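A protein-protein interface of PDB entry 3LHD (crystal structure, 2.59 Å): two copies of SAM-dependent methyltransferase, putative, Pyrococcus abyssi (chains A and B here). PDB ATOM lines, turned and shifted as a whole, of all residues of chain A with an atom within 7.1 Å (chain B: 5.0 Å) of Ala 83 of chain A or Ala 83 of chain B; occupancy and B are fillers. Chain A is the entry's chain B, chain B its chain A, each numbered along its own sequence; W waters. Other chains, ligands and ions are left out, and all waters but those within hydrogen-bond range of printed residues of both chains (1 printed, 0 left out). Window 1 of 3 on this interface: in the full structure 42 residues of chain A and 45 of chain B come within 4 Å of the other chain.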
ATOM      1  N   VAL A  77      40.833   0.323  25.829  1.00  0.00           N
ATOM      2  CA  VAL A  77      39.755  -0.504  25.298  1.00  0.00           C
ATOM      3  C   VAL A  77      38.889   0.416  24.449  1.00  0.00           C
ATOM      4  O   VAL A  77      38.344   1.404  24.947  1.00  0.00           O
ATOM      5  CB  VAL A  77      38.919  -1.195  26.400  1.00  0.00           C
ATOM      6  CG1 VAL A  77      37.612  -1.728  25.833  1.00  0.00           C
ATOM      7  CG2 VAL A  77      39.697  -2.330  27.008  1.00  0.00           C
ATOM      8  N   HIS A  78      38.789   0.092  23.163  1.00  0.00           N
ATOM      9  CA  HIS A  78      38.096   0.937  22.194  1.00  0.00           C
ATOM     10  C   HIS A  78      36.592   0.966  22.410  1.00  0.00           C
ATOM     11  O   HIS A  78      36.024  -0.008  22.900  1.00  0.00           O
ATOM     12  CB  HIS A  78      38.431   0.485  20.775  1.00  0.00           C
ATOM     13  CG  HIS A  78      39.865   0.691  20.416  1.00  0.00           C
ATOM     14  ND1 HIS A  78      40.313   1.824  19.775  1.00  0.00           N
ATOM     15  CD2 HIS A  78      40.958  -0.072  20.644  1.00  0.00           C
ATOM     16  CE1 HIS A  78      41.620   1.737  19.600  1.00  0.00           C
ATOM     17  NE2 HIS A  78      42.035   0.594  20.116  1.00  0.00           N
ATOM     18  N   PRO A  79      35.945   2.090  22.047  1.00  0.00           N
ATOM     19  CA  PRO A  79      34.506   2.284  22.259  1.00  0.00           C
ATOM     20  C   PRO A  79      33.617   1.223  21.611  1.00  0.00           C
ATOM     21  O   PRO A  79      32.510   0.991  22.091  1.00  0.00           O
ATOM     22  CB  PRO A  79      34.244   3.658  21.635  1.00  0.00           C
ATOM     23  CG  PRO A  79      35.562   4.351  21.708  1.00  0.00           C
ATOM     24  CD  PRO A  79      36.560   3.278  21.428  1.00  0.00           C
ATOM     25  N   LYS A  80      34.092   0.583  20.544  1.00  0.00           N
ATOM     26  CA  LYS A  80      33.357  -0.533  19.942  1.00  0.00           C
ATOM     27  C   LYS A  80      33.264  -1.740  20.879  1.00  0.00           C
ATOM     28  O   LYS A  80      32.224  -2.399  20.946  1.00  0.00           O
ATOM     29  CB  LYS A  80      33.957  -0.951  18.594  1.00  0.00           C
ATOM     30  CG  LYS A  80      35.433  -1.288  18.627  1.00  0.00           C
ATOM     31  CD  LYS A  80      35.777  -2.351  17.610  1.00  0.00           C
ATOM     32  CE  LYS A  80      37.180  -2.860  17.853  1.00  0.00           C
ATOM     33  NZ  LYS A  80      37.439  -4.206  17.282  1.00  0.00           N
ATOM     34  N   ASP A  81      34.351  -2.015  21.599  1.00  0.00           N
ATOM     35  CA  ASP A  81      34.408  -3.132  22.535  1.00  0.00           C
ATOM     36  C   ASP A  81      33.555  -2.867  23.773  1.00  0.00           C
ATOM     37  O   ASP A  81      32.864  -3.758  24.262  1.00  0.00           O
ATOM     38  CB  ASP A  81      35.855  -3.409  22.941  1.00  0.00           C
ATOM     39  CG  ASP A  81      36.760  -3.666  21.749  1.00  0.00           C
ATOM     40  OD1 ASP A  81      36.327  -4.362  20.804  1.00  0.00           O
ATOM     41  OD2 ASP A  81      37.910  -3.175  21.763  1.00  0.00           O
ATOM     42  N   ALA A  82      33.609  -1.632  24.259  1.00  0.00           N
ATOM     43  CA  ALA A  82      32.839  -1.201  25.420  1.00  0.00           C
ATOM     44  C   ALA A  82      31.333  -1.193  25.146  1.00  0.00           C
ATOM     45  O   ALA A  82      30.536  -1.519  26.028  1.00  0.00           O
ATOM     46  CB  ALA A  82      33.308   0.162  25.871  1.00  0.00           C
ATOM     47  N   ALA A  83      30.947  -0.821  23.924  1.00  0.00           N
ATOM     48  CA  ALA A  83      29.544  -0.879  23.492  1.00  0.00           C
ATOM     49  C   ALA A  83      29.000  -2.290  23.586  1.00  0.00           C
ATOM     50  O   ALA A  83      27.914  -2.504  24.125  1.00  0.00           O
ATOM     51  CB  ALA A  83      29.401  -0.374  22.073  1.00  0.00           C
ATOM     52  N   LEU A  84      29.758  -3.247  23.060  1.00  0.00           N
ATOM     53  CA  LEU A  84      29.337  -4.634  23.052  1.00  0.00           C
ATOM     54  C   LEU A  84      29.349  -5.220  24.458  1.00  0.00           C
ATOM     55  O   LEU A  84      28.528  -6.079  24.783  1.00  0.00           O
ATOM     56  CB  LEU A  84      30.217  -5.461  22.119  1.00  0.00           C
ATOM     57  CG  LEU A  84      29.742  -5.777  20.696  1.00  0.00           C
ATOM     58  CD1 LEU A  84      28.438  -6.578  20.690  1.00  0.00           C
ATOM     59  CD2 LEU A  84      29.607  -4.551  19.817  1.00  0.00           C
ATOM     60  N   ILE A  85      30.276  -4.756  25.288  1.00  0.00           N
ATOM     61  CA  ILE A  85      30.285  -5.147  26.684  1.00  0.00           C
ATOM     62  C   ILE A  85      28.988  -4.660  27.338  1.00  0.00           C
ATOM     63  O   ILE A  85      28.284  -5.437  27.982  1.00  0.00           O
ATOM     64  CB  ILE A  85      31.529  -4.620  27.420  1.00  0.00           C
ATOM     65  CG1 ILE A  85      32.751  -5.446  27.030  1.00  0.00           C
ATOM     66  CG2 ILE A  85      31.319  -4.626  28.933  1.00  0.00           C
ATOM     67  CD1 ILE A  85      34.061  -4.875  27.529  1.00  0.00           C
ATOM     68  N   VAL A  86      28.661  -3.386  27.140  1.00  0.00           N
ATOM     69  CA  VAL A  86      27.422  -2.831  27.667  1.00  0.00           C
ATOM     70  C   VAL A  86      26.210  -3.605  27.146  1.00  0.00           C
ATOM     71  O   VAL A  86      25.378  -4.053  27.934  1.00  0.00           O
ATOM     72  CB  VAL A  86      27.294  -1.311  27.362  1.00  0.00           C
ATOM     73  CG1 VAL A  86      25.862  -0.847  27.481  1.00  0.00           C
ATOM     74  CG2 VAL A  86      28.180  -0.503  28.302  1.00  0.00           C
ATOM     75  N   ALA A  87      26.128  -3.786  25.828  1.00  0.00           N
ATOM     76  CA  ALA A  87      24.947  -4.394  25.208  1.00  0.00           C
ATOM     77  C   ALA A  87      24.754  -5.863  25.582  1.00  0.00           C
ATOM     78  O   ALA A  87      23.656  -6.279  25.947  1.00  0.00           O
ATOM     79  CB  ALA A  87      24.995  -4.231  23.689  1.00  0.00           C
ATOM     80  N   TYR A  88      25.818  -6.649  25.490  1.00  0.00           N
ATOM     81  CA  TYR A  88      25.691  -8.083  25.732  1.00  0.00           C
ATOM     82  C   TYR A  88      25.504  -8.411  27.205  1.00  0.00           C
ATOM     83  O   TYR A  88      24.703  -9.285  27.541  1.00  0.00           O
ATOM     84  CB  TYR A  88      26.858  -8.860  25.113  1.00  0.00           C
ATOM     85  CG  TYR A  88      26.704  -9.133  23.625  1.00  0.00           C
ATOM     86  CD1 TYR A  88      25.756  -8.451  22.853  1.00  0.00           C
ATOM     87  CD2 TYR A  88      27.517 -10.061  22.987  1.00  0.00           C
ATOM     88  CE1 TYR A  88      25.614  -8.705  21.486  1.00  0.00           C
ATOM     89  CE2 TYR A  88      27.392 -10.317  21.622  1.00  0.00           C
ATOM     90  CZ  TYR A  88      26.440  -9.638  20.875  1.00  0.00           C
ATOM     91  OH  TYR A  88      26.319  -9.899  19.518  1.00  0.00           O
ATOM     92  N   ALA A  89      26.212  -7.689  28.073  1.00  0.00           N
ATOM     93  CA  ALA A  89      26.130  -7.906  29.519  1.00  0.00           C
ATOM     94  C   ALA A  89      24.988  -7.115  30.175  1.00  0.00           C
ATOM     95  O   ALA A  89      24.723  -7.268  31.374  1.00  0.00           O
ATOM     96  CB  ALA A  89      27.458  -7.588  30.178  1.00  0.00           C
ATOM     97  N   LEU A 107      37.769   3.071  29.546  1.00  0.00           N
ATOM     98  CA  LEU A 107      36.696   2.117  29.826  1.00  0.00           C
ATOM     99  C   LEU A 107      35.840   2.618  30.990  1.00  0.00           C
ATOM    100  O   LEU A 107      34.613   2.597  30.940  1.00  0.00           O
ATOM    101  CB  LEU A 107      37.267   0.733  30.146  1.00  0.00           C
ATOM    102  CG  LEU A 107      36.261  -0.392  30.371  1.00  0.00           C
ATOM    103  CD1 LEU A 107      35.149  -0.410  29.303  1.00  0.00           C
ATOM    104  CD2 LEU A 107      36.965  -1.737  30.422  1.00  0.00           C
ATOM    105  N   PHE A 110      33.414   5.343  30.031  1.00  0.00           N
ATOM    106  CA  PHE A 110      32.299   4.777  29.267  1.00  0.00           C
ATOM    107  C   PHE A 110      31.231   4.160  30.164  1.00  0.00           C
ATOM    108  O   PHE A 110      30.064   4.533  30.083  1.00  0.00           O
ATOM    109  CB  PHE A 110      32.806   3.729  28.270  1.00  0.00           C
ATOM    110  CG  PHE A 110      31.780   3.323  27.250  1.00  0.00           C
ATOM    111  CD1 PHE A 110      31.604   4.079  26.086  1.00  0.00           C
ATOM    112  CD2 PHE A 110      30.981   2.203  27.453  1.00  0.00           C
ATOM    113  CE1 PHE A 110      30.646   3.729  25.135  1.00  0.00           C
ATOM    114  CE2 PHE A 110      30.016   1.839  26.510  1.00  0.00           C
ATOM    115  CZ  PHE A 110      29.844   2.605  25.347  1.00  0.00           C
ATOM    116  N   PHE A 249      32.258 -13.402  27.781  1.00  0.00           N
ATOM    117  CA  PHE A 249      31.161 -13.139  28.702  1.00  0.00           C
ATOM    118  C   PHE A 249      30.810 -14.395  29.490  1.00  0.00           C
ATOM    119  O   PHE A 249      30.759 -15.492  28.930  1.00  0.00           O
ATOM    120  CB  PHE A 249      29.915 -12.679  27.943  1.00  0.00           C
ATOM    121  CG  PHE A 249      30.054 -11.347  27.285  1.00  0.00           C
ATOM    122  CD1 PHE A 249      30.577 -11.239  26.006  1.00  0.00           C
ATOM    123  CD2 PHE A 249      29.629 -10.191  27.934  1.00  0.00           C
ATOM    124  CE1 PHE A 249      30.689  -9.995  25.385  1.00  0.00           C
ATOM    125  CE2 PHE A 249      29.740  -8.941  27.317  1.00  0.00           C
ATOM    126  CZ  PHE A 249      30.272  -8.851  26.042  1.00  0.00           C
ATOM    127  N   PRO B  79      21.118  -6.366  18.659  1.00  0.00           N
ATOM    128  CA  PRO B  79      21.879  -5.915  19.823  1.00  0.00           C
ATOM    129  C   PRO B  79      23.204  -5.242  19.462  1.00  0.00           C
ATOM    130  O   PRO B  79      23.488  -4.145  19.951  1.00  0.00           O
ATOM    131  CB  PRO B  79      22.136  -7.216  20.601  1.00  0.00           C
ATOM    132  CG  PRO B  79      21.345  -8.299  19.903  1.00  0.00           C
ATOM    133  CD  PRO B  79      20.420  -7.628  18.948  1.00  0.00           C
ATOM    134  N   LYS B  80      23.989  -5.878  18.596  1.00  0.00           N
ATOM    135  CA  LYS B  80      25.241  -5.295  18.130  1.00  0.00           C
ATOM    136  C   LYS B  80      25.068  -3.913  17.484  1.00  0.00           C
ATOM    137  O   LYS B  80      25.931  -3.048  17.618  1.00  0.00           O
ATOM    138  CB  LYS B  80      25.973  -6.246  17.178  1.00  0.00           C
ATOM    139  CG  LYS B  80      25.218  -6.612  15.898  1.00  0.00           C
ATOM    140  CD  LYS B  80      26.129  -7.350  14.926  1.00  0.00           C
ATOM    141  CE  LYS B  80      25.498  -7.507  13.561  1.00  0.00           C
ATOM    142  NZ  LYS B  80      25.470  -6.234  12.789  1.00  0.00           N
ATOM    143  N   ASP B  81      23.961  -3.706  16.781  1.00  0.00           N
ATOM    144  CA  ASP B  81      23.738  -2.432  16.108  1.00  0.00           C
ATOM    145  C   ASP B  81      23.258  -1.377  17.106  1.00  0.00           C
ATOM    146  O   ASP B  81      23.703  -0.227  17.069  1.00  0.00           O
ATOM    147  CB  ASP B  81      22.771  -2.598  14.929  1.00  0.00           C
ATOM    148  CG  ASP B  81      23.167  -3.744  14.011  1.00  0.00           C
ATOM    149  OD1 ASP B  81      24.315  -3.748  13.520  1.00  0.00           O
ATOM    150  OD2 ASP B  81      22.329  -4.645  13.789  1.00  0.00           O
ATOM    151  N   ALA B  82      22.375  -1.786  18.010  1.00  0.00           N
ATOM    152  CA  ALA B  82      21.978  -0.955  19.137  1.00  0.00           C
ATOM    153  C   ALA B  82      23.209  -0.466  19.911  1.00  0.00           C
ATOM    154  O   ALA B  82      23.299   0.709  20.272  1.00  0.00           O
ATOM    155  CB  ALA B  82      21.050  -1.729  20.048  1.00  0.00           C
ATOM    156  N   ALA B  83      24.161  -1.371  20.131  1.00  0.00           N
ATOM    157  CA  ALA B  83      25.387  -1.076  20.871  1.00  0.00           C
ATOM    158  C   ALA B  83      26.164   0.099  20.302  1.00  0.00           C
ATOM    159  O   ALA B  83      26.565   1.003  21.046  1.00  0.00           O
ATOM    160  CB  ALA B  83      26.277  -2.310  20.919  1.00  0.00           C
ATOM    161  N   LEU B  84      26.391   0.085  18.990  1.00  0.00           N
ATOM    162  CA  LEU B  84      27.211   1.117  18.356  1.00  0.00           C
ATOM    163  C   LEU B  84      26.465   2.444  18.273  1.00  0.00           C
ATOM    164  O   LEU B  84      27.062   3.509  18.390  1.00  0.00           O
ATOM    165  CB  LEU B  84      27.698   0.666  16.980  1.00  0.00           C
ATOM    166  CG  LEU B  84      28.925  -0.257  16.877  1.00  0.00           C
ATOM    167  CD1 LEU B  84      30.216   0.486  17.190  1.00  0.00           C
ATOM    168  CD2 LEU B  84      28.816  -1.510  17.738  1.00  0.00           C
ATOM    169  N   ILE B  85      25.155   2.369  18.083  1.00  0.00           N
ATOM    170  CA  ILE B  85      24.300   3.547  18.139  1.00  0.00           C
ATOM    171  C   ILE B  85      24.497   4.238  19.490  1.00  0.00           C
ATOM    172  O   ILE B  85      24.802   5.433  19.551  1.00  0.00           O
ATOM    173  CB  ILE B  85      22.819   3.171  17.873  1.00  0.00           C
ATOM    174  CG1 ILE B  85      22.639   2.815  16.386  1.00  0.00           C
ATOM    175  CG2 ILE B  85      21.887   4.299  18.292  1.00  0.00           C
ATOM    176  CD1 ILE B  85      21.399   1.969  16.063  1.00  0.00           C
ATOM    177  N   VAL B  86      24.362   3.467  20.564  1.00  0.00           N
ATOM    178  CA  VAL B  86      24.648   3.959  21.907  1.00  0.00           C
ATOM    179  C   VAL B  86      26.062   4.554  21.972  1.00  0.00           C
ATOM    180  O   VAL B  86      26.236   5.720  22.342  1.00  0.00           O
ATOM    181  CB  VAL B  86      24.452   2.851  22.960  1.00  0.00           C
ATOM    182  CG1 VAL B  86      25.035   3.266  24.303  1.00  0.00           C
ATOM    183  CG2 VAL B  86      22.965   2.514  23.102  1.00  0.00           C
ATOM    184  N   ALA B  87      27.053   3.763  21.558  1.00  0.00           N
ATOM    185  CA  ALA B  87      28.455   4.150  21.634  1.00  0.00           C
ATOM    186  C   ALA B  87      28.802   5.412  20.850  1.00  0.00           C
ATOM    187  O   ALA B  87      29.384   6.347  21.405  1.00  0.00           O
ATOM    188  CB  ALA B  87      29.337   3.000  21.174  1.00  0.00           C
ATOM    189  N   PHE B 110      15.821  -1.446  24.544  1.00  0.00           N
ATOM    190  CA  PHE B 110      17.244  -1.226  24.731  1.00  0.00           C
ATOM    191  C   PHE B 110      17.597   0.250  24.970  1.00  0.00           C
ATOM    192  O   PHE B 110      18.402   0.566  25.847  1.00  0.00           O
ATOM    193  CB  PHE B 110      17.997  -1.783  23.522  1.00  0.00           C
ATOM    194  CG  PHE B 110      19.485  -1.748  23.657  1.00  0.00           C
ATOM    195  CD1 PHE B 110      20.176  -2.856  24.142  1.00  0.00           C
ATOM    196  CD2 PHE B 110      20.204  -0.621  23.285  1.00  0.00           C
ATOM    197  CE1 PHE B 110      21.560  -2.834  24.266  1.00  0.00           C
ATOM    198  CE2 PHE B 110      21.590  -0.591  23.403  1.00  0.00           C
ATOM    199  CZ  PHE B 110      22.266  -1.694  23.893  1.00  0.00           C
HETATM  200  O   HOH W   1      24.013  -9.046  18.109  1.00  0.00           O
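Water W1 bridges OH of Tyr 88 of chain A (2.8 Å) and N of Lys 80 of chain B (3.2 Å).
Among the printed residues, merely in contact across the chains: Pro 79 of chain A with Ala 87 of chain B, Ala 83 of chain A with Ala 83 of chain B, Ala 83 of chain A with Ala 87 of chain B, Leu 84 of chain A with Leu 84 of chain B, Ala 87 of chain A with Ala 83 of chain B, Ala 87 of chain A with Phe 110 of chain B and Tyr 88 of chain A with Pro 79 of chain B.
Printed residues of chain B within 4 Å of Ala 83 of chain A: Ala 83 and Ala 87. Of chain A, only Ala 83 and Ala 87 come within 4 Å of Ala 83 of chain B. Printed residues of chain A within 4 Å of Pro 79 of chain B: Tyr 88 (3.9 Å). Of the printed residues of chain B, Tyr 88 of chain A touches Pro 79 (3.9 Å). Of the printed residues of chain A, Leu 84 of chain B touches Leu 84 (3.8 Å). Printed residues of chain B within 4 Å of Ala 87 of chain A: Ala 83 and Phe 110. Of the printed residues of chain B, Leu 84 of chain A touches Leu 84. Ala 82 of chain B touches none of the printed residues of chain A. The nearest residue of chain A that does not touch Ala 83 of chain B is Leu 84 of chain A (4.2 Å).
Pro 79 of chain A touches Ala 87 of chain B, but with the chains exchanged Ala 87 of chain A does not touch Pro 79 of chain B (4.03 Å). Ala 83 of chain B touches its own counterpart, Ala 83 of chain A. Leu 84 of chain B touches its own counterpart, Leu 84 of chain A. Ala 87 of chain A touches Phe 110 of chain B, but with the chains exchanged Phe 110 of chain A does not touch Ala 87 of chain B (4.2 Å). Of the 7 pairs that touch across the chains among the printed residues, 4 have their exchanged pair printed and touching as well.
Printed residues of chain B that touch a printed residue of chain A: Pro 79, Ala 83, Leu 84, Ala 87 and Phe 110. Hydrophobic or aromatic side chains of chain B that line the printed part of chain A: Pro 79, Ala 83, Leu 84, Ala 87 and Phe 110. Among the printed residues, 7 pairs touch across the chains. Among the printed residues, no Asp or Glu carboxylate lies within 4 Å of a Lys or Arg side-chain nitrogen of the other chain.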
